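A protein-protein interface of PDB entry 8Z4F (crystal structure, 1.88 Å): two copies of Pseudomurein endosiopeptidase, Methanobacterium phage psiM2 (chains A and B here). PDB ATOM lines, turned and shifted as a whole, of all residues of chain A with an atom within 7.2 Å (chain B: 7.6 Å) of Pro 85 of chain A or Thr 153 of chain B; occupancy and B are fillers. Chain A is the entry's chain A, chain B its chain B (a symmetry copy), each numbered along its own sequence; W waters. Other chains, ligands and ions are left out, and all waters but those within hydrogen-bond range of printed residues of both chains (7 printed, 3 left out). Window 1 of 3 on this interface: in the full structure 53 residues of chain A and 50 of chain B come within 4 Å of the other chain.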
ATOM      1  N   GLU A  82     -10.264  -0.785  15.970  1.00  0.00           N
ATOM      2  CA  GLU A  82      -9.559  -0.477  14.733  1.00  0.00           C
ATOM      3  C   GLU A  82      -9.905  -1.551  13.716  1.00  0.00           C
ATOM      4  O   GLU A  82      -9.772  -2.748  14.005  1.00  0.00           O
ATOM      5  CB  GLU A  82      -8.045  -0.398  14.956  1.00  0.00           C
ATOM      6  CG  GLU A  82      -7.552   0.895  15.727  1.00  0.00           C
ATOM      7  CD  GLU A  82      -6.031   0.908  15.786  1.00  0.00           C
ATOM      8  OE1 GLU A  82      -5.457  -0.123  16.186  1.00  0.00           O
ATOM      9  OE2 GLU A  82      -5.392   1.927  15.425  1.00  0.00           O
ATOM     10  N   ASN A  83     -10.374  -1.127  12.552  1.00  0.00           N
ATOM     11  CA  ASN A  83     -10.624  -2.032  11.433  1.00  0.00           C
ATOM     12  C   ASN A  83      -9.376  -2.182  10.576  1.00  0.00           C
ATOM     13  O   ASN A  83      -8.578  -1.251  10.442  1.00  0.00           O
ATOM     14  CB  ASN A  83     -11.743  -1.510  10.539  1.00  0.00           C
ATOM     15  CG  ASN A  83     -13.092  -1.562  11.199  1.00  0.00           C
ATOM     16  OD1 ASN A  83     -13.563  -2.619  11.565  1.00  0.00           O
ATOM     17  ND2 ASN A  83     -13.720  -0.403  11.358  1.00  0.00           N
ATOM     18  N   THR A  84      -9.232  -3.349   9.963  1.00  0.00           N
ATOM     19  CA  THR A  84      -8.280  -3.470   8.874  1.00  0.00           C
ATOM     20  C   THR A  84      -8.652  -2.467   7.780  1.00  0.00           C
ATOM     21  O   THR A  84      -9.796  -2.479   7.313  1.00  0.00           O
ATOM     22  CB  THR A  84      -8.281  -4.876   8.294  1.00  0.00           C
ATOM     23  OG1 THR A  84      -8.045  -5.831   9.363  1.00  0.00           O
ATOM     24  CG2 THR A  84      -7.183  -4.996   7.217  1.00  0.00           C
ATOM     25  N   PRO A  85      -7.750  -1.576   7.386  1.00  0.00           N
ATOM     26  CA  PRO A  85      -8.118  -0.462   6.500  1.00  0.00           C
ATOM     27  C   PRO A  85      -8.108  -0.843   5.028  1.00  0.00           C
ATOM     28  O   PRO A  85      -7.445  -1.790   4.609  1.00  0.00           O
ATOM     29  CB  PRO A  85      -7.024   0.579   6.779  1.00  0.00           C
ATOM     30  CG  PRO A  85      -5.810  -0.276   7.053  1.00  0.00           C
ATOM     31  CD  PRO A  85      -6.370  -1.465   7.885  1.00  0.00           C
ATOM     32  N   GLU A  86      -8.822  -0.030   4.230  1.00  0.00           N
ATOM     33  CA  GLU A  86      -8.847  -0.237   2.784  1.00  0.00           C
ATOM     34  C   GLU A  86      -7.467  -0.037   2.163  1.00  0.00           C
ATOM     35  O   GLU A  86      -7.125  -0.695   1.163  1.00  0.00           O
ATOM     36  CB  GLU A  86      -9.865   0.713   2.124  1.00  0.00           C
ATOM     37  CG  GLU A  86     -10.122   0.365   0.650  1.00  0.00           C
ATOM     38  CD  GLU A  86     -10.944   1.418  -0.124  1.00  0.00           C
ATOM     39  OE1 GLU A  86     -11.056   2.562   0.323  1.00  0.00           O
ATOM     40  OE2 GLU A  86     -11.473   1.068  -1.201  1.00  0.00           O
ATOM     41  N   TYR A  87      -6.660   0.858   2.738  1.00  0.00           N
ATOM     42  CA  TYR A  87      -5.329   1.175   2.237  1.00  0.00           C
ATOM     43  C   TYR A  87      -4.458   1.563   3.414  1.00  0.00           C
ATOM     44  O   TYR A  87      -4.954   1.857   4.506  1.00  0.00           O
ATOM     45  CB  TYR A  87      -5.334   2.340   1.216  1.00  0.00           C
ATOM     46  CG  TYR A  87      -6.039   3.570   1.785  1.00  0.00           C
ATOM     47  CD1 TYR A  87      -5.403   4.409   2.702  1.00  0.00           C
ATOM     48  CD2 TYR A  87      -7.345   3.862   1.429  1.00  0.00           C
ATOM     49  CE1 TYR A  87      -6.056   5.514   3.250  1.00  0.00           C
ATOM     50  CE2 TYR A  87      -8.019   4.965   1.982  1.00  0.00           C
ATOM     51  CZ  TYR A  87      -7.361   5.791   2.880  1.00  0.00           C
ATOM     52  OH  TYR A  87      -8.020   6.893   3.415  1.00  0.00           O
ATOM     53  N   VAL A  88      -3.149   1.589   3.171  1.00  0.00           N
ATOM     54  CA  VAL A  88      -2.173   2.120   4.119  1.00  0.00           C
ATOM     55  C   VAL A  88      -1.339   3.157   3.381  1.00  0.00           C
ATOM     56  O   VAL A  88      -1.165   3.085   2.163  1.00  0.00           O
ATOM     57  CB  VAL A  88      -1.243   1.036   4.698  1.00  0.00           C
ATOM     58  CG1 VAL A  88      -2.030  -0.003   5.508  1.00  0.00           C
ATOM     59  CG2 VAL A  88      -0.449   0.334   3.559  1.00  0.00           C
ATOM     60  N   ILE A 116      -0.803  -4.454  10.638  1.00  0.00           N
ATOM     61  CA  ILE A 116      -0.685  -3.095  10.091  1.00  0.00           C
ATOM     62  C   ILE A 116       0.316  -2.287  10.915  1.00  0.00           C
ATOM     63  O   ILE A 116       1.288  -1.723  10.387  1.00  0.00           O
ATOM     64  CB  ILE A 116      -2.055  -2.394  10.055  1.00  0.00           C
ATOM     65  CG1 ILE A 116      -3.070  -3.162   9.210  1.00  0.00           C
ATOM     66  CG2 ILE A 116      -1.906  -0.902   9.569  1.00  0.00           C
ATOM     67  CD1 ILE A 116      -2.790  -3.171   7.708  1.00  0.00           C
ATOM     68  N   TYR A 117       0.095  -2.234  12.224  1.00  0.00           N
ATOM     69  CA  TYR A 117       0.974  -1.535  13.147  1.00  0.00           C
ATOM     70  C   TYR A 117       1.791  -2.528  13.960  1.00  0.00           C
ATOM     71  O   TYR A 117       1.314  -3.607  14.322  1.00  0.00           O
ATOM     72  CB  TYR A 117       0.168  -0.682  14.119  1.00  0.00           C
ATOM     73  CG  TYR A 117      -0.750   0.283  13.469  1.00  0.00           C
ATOM     74  CD1 TYR A 117      -0.281   1.484  12.975  1.00  0.00           C
ATOM     75  CD2 TYR A 117      -2.095   0.001  13.352  1.00  0.00           C
ATOM     76  CE1 TYR A 117      -1.132   2.386  12.377  1.00  0.00           C
ATOM     77  CE2 TYR A 117      -2.969   0.913  12.759  1.00  0.00           C
ATOM     78  CZ  TYR A 117      -2.474   2.093  12.280  1.00  0.00           C
ATOM     79  OH  TYR A 117      -3.345   2.991  11.706  1.00  0.00           O
ATOM     80  N   PRO A 122      -5.036  -4.531  13.950  1.00  0.00           N
ATOM     81  CA  PRO A 122      -5.523  -5.166  12.724  1.00  0.00           C
ATOM     82  C   PRO A 122      -4.351  -5.774  11.963  1.00  0.00           C
ATOM     83  O   PRO A 122      -3.204  -5.362  12.128  1.00  0.00           O
ATOM     84  CB  PRO A 122      -6.161  -4.012  11.935  1.00  0.00           C
ATOM     85  CG  PRO A 122      -5.767  -2.744  12.632  1.00  0.00           C
ATOM     86  CD  PRO A 122      -5.342  -3.086  14.021  1.00  0.00           C
ATOM     87  N   SER A 123      -4.644  -6.776  11.133  1.00  0.00           N
ATOM     88  CA  SER A 123      -3.605  -7.452  10.361  1.00  0.00           C
ATOM     89  C   SER A 123      -4.185  -7.839   9.007  1.00  0.00           C
ATOM     90  O   SER A 123      -5.400  -7.863   8.822  1.00  0.00           O
ATOM     91  CB  SER A 123      -3.064  -8.680  11.097  1.00  0.00           C
ATOM     92  OG  SER A 123      -3.976  -9.765  11.005  1.00  0.00           O
ATOM     93  N   VAL A 124      -3.311  -8.116   8.050  1.00  0.00           N
ATOM     94  CA  VAL A 124      -3.737  -8.685   6.769  1.00  0.00           C
ATOM     95  C   VAL A 124      -3.160 -10.087   6.679  1.00  0.00           C
ATOM     96  O   VAL A 124      -2.154 -10.410   7.325  1.00  0.00           O
ATOM     97  CB  VAL A 124      -3.339  -7.829   5.544  1.00  0.00           C
ATOM     98  CG1 VAL A 124      -3.932  -6.362   5.666  1.00  0.00           C
ATOM     99  CG2 VAL A 124      -1.817  -7.776   5.372  1.00  0.00           C
ATOM    100  N   MET A 132      -0.350  -6.945  -1.928  1.00  0.00           N
ATOM    101  CA  MET A 132       0.000  -5.519  -1.753  1.00  0.00           C
ATOM    102  C   MET A 132       1.389  -5.275  -2.347  1.00  0.00           C
ATOM    103  O   MET A 132       1.563  -4.328  -3.075  1.00  0.00           O
ATOM    104  CB  MET A 132       0.012  -5.161  -0.268  1.00  0.00           C
ATOM    105  CG  MET A 132      -1.360  -5.109   0.327  1.00  0.00           C
ATOM    106  SD  MET A 132      -1.359  -4.921   2.097  1.00  0.00           S
ATOM    107  CE  MET A 132      -0.937  -3.196   2.282  1.00  0.00           C
ATOM    108  N   VAL A 150      -0.915   2.461  -0.515  1.00  0.00           N
ATOM    109  CA  VAL A 150      -0.912   1.099  -1.053  1.00  0.00           C
ATOM    110  C   VAL A 150      -2.224   0.474  -0.586  1.00  0.00           C
ATOM    111  O   VAL A 150      -2.480   0.407   0.630  1.00  0.00           O
ATOM    112  CB  VAL A 150       0.291   0.280  -0.546  1.00  0.00           C
ATOM    113  CG1 VAL A 150       0.159  -1.207  -0.938  1.00  0.00           C
ATOM    114  CG2 VAL A 150       1.643   0.869  -1.029  1.00  0.00           C
ATOM    115  N   TYR A 151      -3.073   0.066  -1.534  1.00  0.00           N
ATOM    116  CA  TYR A 151      -4.371  -0.485  -1.167  1.00  0.00           C
ATOM    117  C   TYR A 151      -4.195  -1.887  -0.596  1.00  0.00           C
ATOM    118  O   TYR A 151      -3.471  -2.706  -1.172  1.00  0.00           O
ATOM    119  CB  TYR A 151      -5.297  -0.548  -2.366  1.00  0.00           C
ATOM    120  CG  TYR A 151      -5.903   0.799  -2.666  1.00  0.00           C
ATOM    121  CD1 TYR A 151      -6.991   1.258  -1.957  1.00  0.00           C
ATOM    122  CD2 TYR A 151      -5.349   1.617  -3.631  1.00  0.00           C
ATOM    123  CE1 TYR A 151      -7.539   2.522  -2.213  1.00  0.00           C
ATOM    124  CE2 TYR A 151      -5.886   2.862  -3.908  1.00  0.00           C
ATOM    125  CZ  TYR A 151      -6.973   3.304  -3.193  1.00  0.00           C
ATOM    126  OH  TYR A 151      -7.505   4.549  -3.469  1.00  0.00           O
ATOM    127  N   VAL A 152      -4.833  -2.117   0.555  1.00  0.00           N
ATOM    128  CA  VAL A 152      -5.043  -3.469   1.070  1.00  0.00           C
ATOM    129  C   VAL A 152      -6.014  -4.211   0.171  1.00  0.00           C
ATOM    130  O   VAL A 152      -5.733  -5.326  -0.276  1.00  0.00           O
ATOM    131  CB  VAL A 152      -5.553  -3.400   2.519  1.00  0.00           C
ATOM    132  CG1 VAL A 152      -5.807  -4.836   3.094  1.00  0.00           C
ATOM    133  CG2 VAL A 152      -4.540  -2.651   3.352  1.00  0.00           C
ATOM    134  N   THR A 153      -7.140  -3.576  -0.149  1.00  0.00           N
ATOM    135  CA  THR A 153      -8.124  -4.118  -1.080  1.00  0.00           C
ATOM    136  C   THR A 153      -8.391  -3.043  -2.134  1.00  0.00           C
ATOM    137  O   THR A 153      -8.972  -1.991  -1.797  1.00  0.00           O
ATOM    138  CB  THR A 153      -9.413  -4.499  -0.345  1.00  0.00           C
ATOM    139  OG1 THR A 153      -9.970  -3.348   0.302  1.00  0.00           O
ATOM    140  CG2 THR A 153      -9.161  -5.582   0.712  1.00  0.00           C
ATOM    141  N   PRO A 154      -7.970  -3.221  -3.387  1.00  0.00           N
ATOM    142  CA  PRO A 154      -8.221  -2.187  -4.412  1.00  0.00           C
ATOM    143  C   PRO A 154      -9.701  -1.877  -4.514  1.00  0.00           C
ATOM    144  O   PRO A 154     -10.536  -2.787  -4.402  1.00  0.00           O
ATOM    145  CB  PRO A 154      -7.692  -2.833  -5.706  1.00  0.00           C
ATOM    146  CG  PRO A 154      -6.621  -3.756  -5.227  1.00  0.00           C
ATOM    147  CD  PRO A 154      -7.130  -4.309  -3.901  1.00  0.00           C
ATOM    148  N   THR B  84      -7.145  -8.736  -3.767  1.00  0.00           N
ATOM    149  CA  THR B  84      -8.013  -9.182  -2.660  1.00  0.00           C
ATOM    150  C   THR B  84      -9.261  -8.296  -2.719  1.00  0.00           C
ATOM    151  O   THR B  84      -9.135  -7.109  -2.801  1.00  0.00           O
ATOM    152  CB  THR B  84      -7.257  -9.459  -1.360  1.00  0.00           C
ATOM    153  OG1 THR B  84      -8.002  -8.896  -0.294  1.00  0.00           O
ATOM    154  CG2 THR B  84      -5.815  -9.030  -1.393  1.00  0.00           C
ATOM    155  N   PRO B  85     -10.463  -8.873  -2.746  1.00  0.00           N
ATOM    156  CA  PRO B  85     -11.669  -8.094  -2.927  1.00  0.00           C
ATOM    157  C   PRO B  85     -12.010  -7.073  -1.842  1.00  0.00           C
ATOM    158  O   PRO B  85     -11.807  -7.360  -0.726  1.00  0.00           O
ATOM    159  CB  PRO B  85     -12.794  -9.124  -2.981  1.00  0.00           C
ATOM    160  CG  PRO B  85     -12.202 -10.392  -2.488  1.00  0.00           C
ATOM    161  CD  PRO B  85     -10.709 -10.284  -2.615  1.00  0.00           C
ATOM    162  N   GLU B  86     -12.505  -5.906  -2.256  1.00  0.00           N
ATOM    163  CA  GLU B  86     -12.980  -4.924  -1.295  1.00  0.00           C
ATOM    164  C   GLU B  86     -14.256  -5.371  -0.600  1.00  0.00           C
ATOM    165  O   GLU B  86     -14.518  -4.963   0.550  1.00  0.00           O
ATOM    166  CB  GLU B  86     -13.205  -3.571  -1.996  1.00  0.00           C
ATOM    167  CG  GLU B  86     -13.603  -2.516  -0.996  1.00  0.00           C
ATOM    168  CD  GLU B  86     -14.095  -1.201  -1.621  1.00  0.00           C
ATOM    169  OE1 GLU B  86     -14.372  -1.169  -2.840  1.00  0.00           O
ATOM    170  OE2 GLU B  86     -14.250  -0.225  -0.849  1.00  0.00           O
ATOM    171  N   TYR B  87     -15.085  -6.161  -1.284  1.00  0.00           N
ATOM    172  CA  TYR B  87     -16.320  -6.662  -0.698  1.00  0.00           C
ATOM    173  C   TYR B  87     -16.654  -8.015  -1.332  1.00  0.00           C
ATOM    174  O   TYR B  87     -16.138  -8.368  -2.397  1.00  0.00           O
ATOM    175  CB  TYR B  87     -17.474  -5.638  -0.871  1.00  0.00           C
ATOM    176  CG  TYR B  87     -17.734  -5.240  -2.314  1.00  0.00           C
ATOM    177  CD1 TYR B  87     -18.232  -6.162  -3.235  1.00  0.00           C
ATOM    178  CD2 TYR B  87     -17.552  -3.914  -2.745  1.00  0.00           C
ATOM    179  CE1 TYR B  87     -18.477  -5.804  -4.557  1.00  0.00           C
ATOM    180  CE2 TYR B  87     -17.814  -3.543  -4.070  1.00  0.00           C
ATOM    181  CZ  TYR B  87     -18.273  -4.498  -4.966  1.00  0.00           C
ATOM    182  OH  TYR B  87     -18.527  -4.168  -6.284  1.00  0.00           O
ATOM    183  N   VAL B 124      -8.367 -13.565   4.161  1.00  0.00           N
ATOM    184  CA  VAL B 124      -8.323 -12.438   5.085  1.00  0.00           C
ATOM    185  C   VAL B 124      -7.874 -12.938   6.442  1.00  0.00           C
ATOM    186  O   VAL B 124      -8.054 -14.115   6.802  1.00  0.00           O
ATOM    187  CB  VAL B 124      -9.671 -11.697   5.204  1.00  0.00           C
ATOM    188  CG1 VAL B 124     -10.202 -11.370   3.817  1.00  0.00           C
ATOM    189  CG2 VAL B 124     -10.715 -12.525   6.014  1.00  0.00           C
ATOM    190  N   THR B 128      -9.596  -9.349  10.344  1.00  0.00           N
ATOM    191  CA  THR B 128     -10.437  -8.781   9.285  1.00  0.00           C
ATOM    192  C   THR B 128     -11.775  -9.507   9.192  1.00  0.00           C
ATOM    193  O   THR B 128     -12.830  -8.883   9.037  1.00  0.00           O
ATOM    194  CB  THR B 128      -9.679  -8.842   7.954  1.00  0.00           C
ATOM    195  OG1 THR B 128      -8.526  -7.967   8.004  1.00  0.00           O
ATOM    196  CG2 THR B 128     -10.588  -8.428   6.799  1.00  0.00           C
ATOM    197  N   ASP B 131     -14.022  -8.154  11.716  1.00  0.00           N
ATOM    198  CA  ASP B 131     -14.559  -6.870  11.226  1.00  0.00           C
ATOM    199  C   ASP B 131     -15.731  -7.113  10.299  1.00  0.00           C
ATOM    200  O   ASP B 131     -16.729  -6.377  10.336  1.00  0.00           O
ATOM    201  CB  ASP B 131     -13.500  -6.100  10.433  1.00  0.00           C
ATOM    202  CG  ASP B 131     -12.332  -5.662  11.264  1.00  0.00           C
ATOM    203  OD1 ASP B 131     -12.418  -5.677  12.518  1.00  0.00           O
ATOM    204  OD2 ASP B 131     -11.315  -5.302  10.641  1.00  0.00           O
ATOM    205  N   MET B 132     -15.605  -8.125   9.413  1.00  0.00           N
ATOM    206  CA  MET B 132     -16.674  -8.373   8.457  1.00  0.00           C
ATOM    207  C   MET B 132     -17.942  -8.801   9.178  1.00  0.00           C
ATOM    208  O   MET B 132     -19.051  -8.337   8.833  1.00  0.00           O
ATOM    209  CB  MET B 132     -16.283  -9.436   7.412  1.00  0.00           C
ATOM    210  CG  MET B 132     -15.185  -8.959   6.411  1.00  0.00           C
ATOM    211  SD  MET B 132     -14.504 -10.303   5.462  1.00  0.00           S
ATOM    212  CE  MET B 132     -15.967 -10.659   4.485  1.00  0.00           C
ATOM    213  N   ARG B 135     -19.661  -5.837  10.622  1.00  0.00           N
ATOM    214  CA  ARG B 135     -20.411  -5.014   9.668  1.00  0.00           C
ATOM    215  C   ARG B 135     -21.746  -5.662   9.297  1.00  0.00           C
ATOM    216  O   ARG B 135     -22.769  -4.969   9.130  1.00  0.00           O
ATOM    217  CB  ARG B 135     -19.571  -4.739   8.412  1.00  0.00           C
ATOM    218  CG  ARG B 135     -18.377  -3.816   8.666  1.00  0.00           C
ATOM    219  CD  ARG B 135     -17.662  -3.330   7.397  1.00  0.00           C
ATOM    220  NE  ARG B 135     -16.620  -4.262   6.999  1.00  0.00           N
ATOM    221  CZ  ARG B 135     -15.366  -4.231   7.435  1.00  0.00           C
ATOM    222  NH1 ARG B 135     -14.926  -3.261   8.235  1.00  0.00           N
ATOM    223  NH2 ARG B 135     -14.553  -5.234   7.110  1.00  0.00           N
ATOM    224  N   VAL B 150     -21.005  -7.660   1.723  1.00  0.00           N
ATOM    225  CA  VAL B 150     -20.300  -7.531   2.988  1.00  0.00           C
ATOM    226  C   VAL B 150     -18.899  -7.031   2.672  1.00  0.00           C
ATOM    227  O   VAL B 150     -18.148  -7.702   1.951  1.00  0.00           O
ATOM    228  CB  VAL B 150     -20.245  -8.868   3.754  1.00  0.00           C
ATOM    229  CG1 VAL B 150     -19.402  -8.691   5.028  1.00  0.00           C
ATOM    230  CG2 VAL B 150     -21.655  -9.333   4.093  1.00  0.00           C
ATOM    231  N   TYR B 151     -18.542  -5.869   3.218  1.00  0.00           N
ATOM    232  CA  TYR B 151     -17.270  -5.229   2.918  1.00  0.00           C
ATOM    233  C   TYR B 151     -16.134  -5.907   3.682  1.00  0.00           C
ATOM    234  O   TYR B 151     -16.241  -6.119   4.881  1.00  0.00           O
ATOM    235  CB  TYR B 151     -17.322  -3.739   3.290  1.00  0.00           C
ATOM    236  CG  TYR B 151     -17.792  -2.924   2.100  1.00  0.00           C
ATOM    237  CD1 TYR B 151     -19.137  -2.855   1.774  1.00  0.00           C
ATOM    238  CD2 TYR B 151     -16.883  -2.316   1.252  1.00  0.00           C
ATOM    239  CE1 TYR B 151     -19.576  -2.123   0.658  1.00  0.00           C
ATOM    240  CE2 TYR B 151     -17.309  -1.606   0.107  1.00  0.00           C
ATOM    241  CZ  TYR B 151     -18.648  -1.521  -0.176  1.00  0.00           C
ATOM    242  OH  TYR B 151     -19.069  -0.822  -1.311  1.00  0.00           O
ATOM    243  N   VAL B 152     -15.023  -6.124   2.991  1.00  0.00           N
ATOM    244  CA  VAL B 152     -13.816  -6.702   3.586  1.00  0.00           C
ATOM    245  C   VAL B 152     -13.055  -5.650   4.353  1.00  0.00           C
ATOM    246  O   VAL B 152     -12.465  -5.945   5.400  1.00  0.00           O
ATOM    247  CB  VAL B 152     -12.929  -7.338   2.498  1.00  0.00           C
ATOM    248  CG1 VAL B 152     -11.588  -7.810   3.084  1.00  0.00           C
ATOM    249  CG2 VAL B 152     -13.642  -8.514   1.830  1.00  0.00           C
ATOM    250  N   THR B 153     -13.028  -4.416   3.840  1.00  0.00           N
ATOM    251  CA  THR B 153     -12.452  -3.273   4.531  1.00  0.00           C
ATOM    252  C   THR B 153     -13.496  -2.164   4.464  1.00  0.00           C
ATOM    253  O   THR B 153     -14.386  -2.200   3.606  1.00  0.00           O
ATOM    254  CB  THR B 153     -11.145  -2.809   3.871  1.00  0.00           C
ATOM    255  OG1 THR B 153     -11.413  -2.485   2.505  1.00  0.00           O
ATOM    256  CG2 THR B 153     -10.041  -3.914   3.910  1.00  0.00           C
ATOM    257  N   PRO B 154     -13.429  -1.178   5.349  1.00  0.00           N
ATOM    258  CA  PRO B 154     -14.511  -0.173   5.415  1.00  0.00           C
ATOM    259  C   PRO B 154     -14.569   0.641   4.137  1.00  0.00           C
ATOM    260  O   PRO B 154     -13.528   1.045   3.606  1.00  0.00           O
ATOM    261  CB  PRO B 154     -14.117   0.702   6.620  1.00  0.00           C
ATOM    262  CG  PRO B 154     -13.129  -0.115   7.395  1.00  0.00           C
ATOM    263  CD  PRO B 154     -12.390  -0.908   6.363  1.00  0.00           C
ATOM    264  N   PRO B 155     -15.764   0.877   3.600  1.00  0.00           N
ATOM    265  CA  PRO B 155     -15.882   1.723   2.411  1.00  0.00           C
ATOM    266  C   PRO B 155     -15.426   3.147   2.715  1.00  0.00           C
ATOM    267  O   PRO B 155     -15.644   3.668   3.812  1.00  0.00           O
ATOM    268  CB  PRO B 155     -17.374   1.660   2.080  1.00  0.00           C
ATOM    269  CG  PRO B 155     -18.036   1.271   3.333  1.00  0.00           C
ATOM    270  CD  PRO B 155     -17.072   0.366   4.047  1.00  0.00           C
ATOM    271  N   GLU B 156     -14.727   3.740   1.759  1.00  0.00           N
ATOM    272  CA  GLU B 156     -14.173   5.081   1.886  1.00  0.00           C
ATOM    273  C   GLU B 156     -14.303   5.777   0.540  1.00  0.00           C
ATOM    274  O   GLU B 156     -14.237   5.124  -0.510  1.00  0.00           O
ATOM    275  CB  GLU B 156     -12.687   5.084   2.287  1.00  0.00           C
ATOM    276  CG  GLU B 156     -12.264   4.102   3.377  1.00  0.00           C
ATOM    277  CD  GLU B 156     -12.524   4.622   4.768  1.00  0.00           C
ATOM    278  OE1 GLU B 156     -13.110   5.720   4.887  1.00  0.00           O
ATOM    279  OE2 GLU B 156     -12.169   3.915   5.748  1.00  0.00           O
ATOM    280  N   LYS B 221      -7.534  12.163   9.078  1.00  0.00           N
ATOM    281  CA  LYS B 221      -6.711  10.963   8.907  1.00  0.00           C
ATOM    282  C   LYS B 221      -6.537  10.589   7.431  1.00  0.00           C
ATOM    283  O   LYS B 221      -5.382  10.421   6.989  1.00  0.00           O
ATOM    284  CB  LYS B 221      -7.276   9.804   9.747  1.00  0.00           C
ATOM    285  CG  LYS B 221      -6.757   8.454   9.241  1.00  0.00           C
ATOM    286  CD  LYS B 221      -6.968   7.327  10.270  1.00  0.00           C
ATOM    287  CE  LYS B 221      -6.441   6.006   9.677  1.00  0.00           C
ATOM    288  NZ  LYS B 221      -6.001   5.057  10.718  1.00  0.00           N
ATOM    289  N   GLU B 225      -2.948  10.580   5.572  1.00  0.00           N
ATOM    290  CA  GLU B 225      -2.453   9.339   4.961  1.00  0.00           C
ATOM    291  C   GLU B 225      -2.204   9.518   3.471  1.00  0.00           C
ATOM    292  O   GLU B 225      -1.208   9.015   2.936  1.00  0.00           O
ATOM    293  CB  GLU B 225      -3.447   8.203   5.203  1.00  0.00           C
ATOM    294  CG  GLU B 225      -3.340   7.686   6.584  1.00  0.00           C
ATOM    295  CD  GLU B 225      -4.202   6.452   6.793  1.00  0.00           C
ATOM    296  OE1 GLU B 225      -5.411   6.491   6.477  1.00  0.00           O
ATOM    297  OE2 GLU B 225      -3.651   5.455   7.258  1.00  0.00           O
HETATM  298  O   HOH W   1      -9.008  -5.866  12.068  1.00  0.00           O
HETATM  299  O   HOH W   2      -8.474   6.647   6.079  1.00  0.00           O
HETATM  300  O   HOH W   3      -5.630   2.583   9.434  1.00  0.00           O
HETATM  301  O   HOH W   4     -10.445   1.918   5.549  1.00  0.00           O
HETATM  302  O   HOH W   5      -4.986   3.358   6.931  1.00  0.00           O
HETATM  303  O   HOH W   6     -16.479  -0.902   9.353  1.00  0.00           O
HETATM  304  O   HOH W   7     -10.480  -5.453  -4.822  1.00  0.00           O
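OD1 of Asp 131 of chain B lies close to OD1 of Asn 83 of chain A (3.4 Å). The side-chain hydroxyl of Thr 84 of chain A is in hydrogen-bond range of the side-chain hydroxyl of Thr 128 of chain B, 2.6 Å away. The backbone NH (N) of Thr 84 of chain A sits at hydrogen-bond distance from the side-chain carboxylate (OD2) of Asp 131 of chain B (2.9 Å). O of Ser 123 of chain A is in hydrogen-bond range of OG1 of Thr 128 of chain B, at 3.2 Å. The side-chain hydroxyl of Thr 153 of chain A lies within hydrogen-bond range of the side-chain hydroxyl of Thr 153 of chain B (2.8 Å). The side-chain carboxylate of Glu 86 of chain A lies close to the side-chain carboxylate of Glu 86 of chain B (3.1 Å).
The backbone carbonyl oxygen of Glu 86 of chain A lies within hydrogen-bond range of the backbone NH of Val 152 of chain A (2.8 Å). The backbone NH (N) of Thr 153 of chain A sits at hydrogen-bond distance from the backbone carbonyl oxygen (O) of Glu 86 of chain A (3.2 Å). NE of Arg 135 of chain B sits at hydrogen-bond distance from O of Tyr 151 of chain B, at 2.8 Å.
Among the printed residues, merely in contact across the chains: Thr 84 of chain A with Pro 154 of chain B, Glu 86 of chain A with Thr 153 of chain B, Pro 85 of chain A with Thr 153 of chain B, Tyr 87 of chain A with Glu 225 of chain B, Thr 153 of chain A with Pro 85 of chain B, Tyr 117 of chain A with Lys 221 of chain B, Glu 86 of chain A with Glu 156 of chain B, Thr 153 of chain A with Thr 84 of chain B, Pro 154 of chain A with Thr 84 of chain B, Asn 83 of chain A with Arg 135 of chain B, Pro 154 of chain A with Glu 86 of chain B, Thr 84 of chain A with Thr 153 of chain B, Asn 83 of chain A with Pro 154 of chain B, Thr 153 of chain A with Glu 86 of chain B, Val 152 of chain A with Thr 84 of chain B and Glu 86 of chain A with Pro 154 of chain B.
Of chain B, only Thr 153 (3.4 Å) comes within 4 Å of Pro 85 of chain A. Printed residues of chain A within 4 Å of Arg 135 of chain B: Asn 83. Printed residues of chain B within 4 Å of Asn 83 of chain A: Asp 131 (3.3 Å), Arg 135 (3.7 Å) and Pro 154 (3.7 Å). Pro 155 of chain B touches none of the printed residues of chain A. Glu 82 of chain A touches none of the printed residues of chain B.
Hydrophobic or aromatic side chains of chain A that line the printed part of chain B: Tyr 87, Tyr 117 and Pro 154. Along chain A the printed residues that touch a printed residue of chain B span positions 83 to 154. Printed residues of chain B that touch a printed residue of chain A: Thr 84, Pro 85, Glu 86, Thr 128, Asp 131, Arg 135, Thr 153, Pro 154, Glu 156, Lys 221 and Glu 225. Among the printed residues, no Asp or Glu carboxylate lies within 4 Å of a Lys or Arg side-chain nitrogen of the other chain.
Glu 86 of chain A touches Pro 154 of chain B, and with the chains exchanged Pro 154 of chain A touches Glu 86 of chain B. Val 152 of chain A touches Thr 84 of chain B, but with the chains exchanged Thr 84 of chain A does not touch Val 152 of chain B (4.8 Å). 11 positions are printed for both chains.
Water W7 lies within hydrogen-bond range of O of Pro 154 of chain A, O of Thr 84 of chain B and N of Glu 86 of chain B. Water W2 lies within hydrogen-bond range of OH of Tyr 87 of chain A (2.7 Å) and OE1 of Glu 225 of chain B (3.1 Å).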
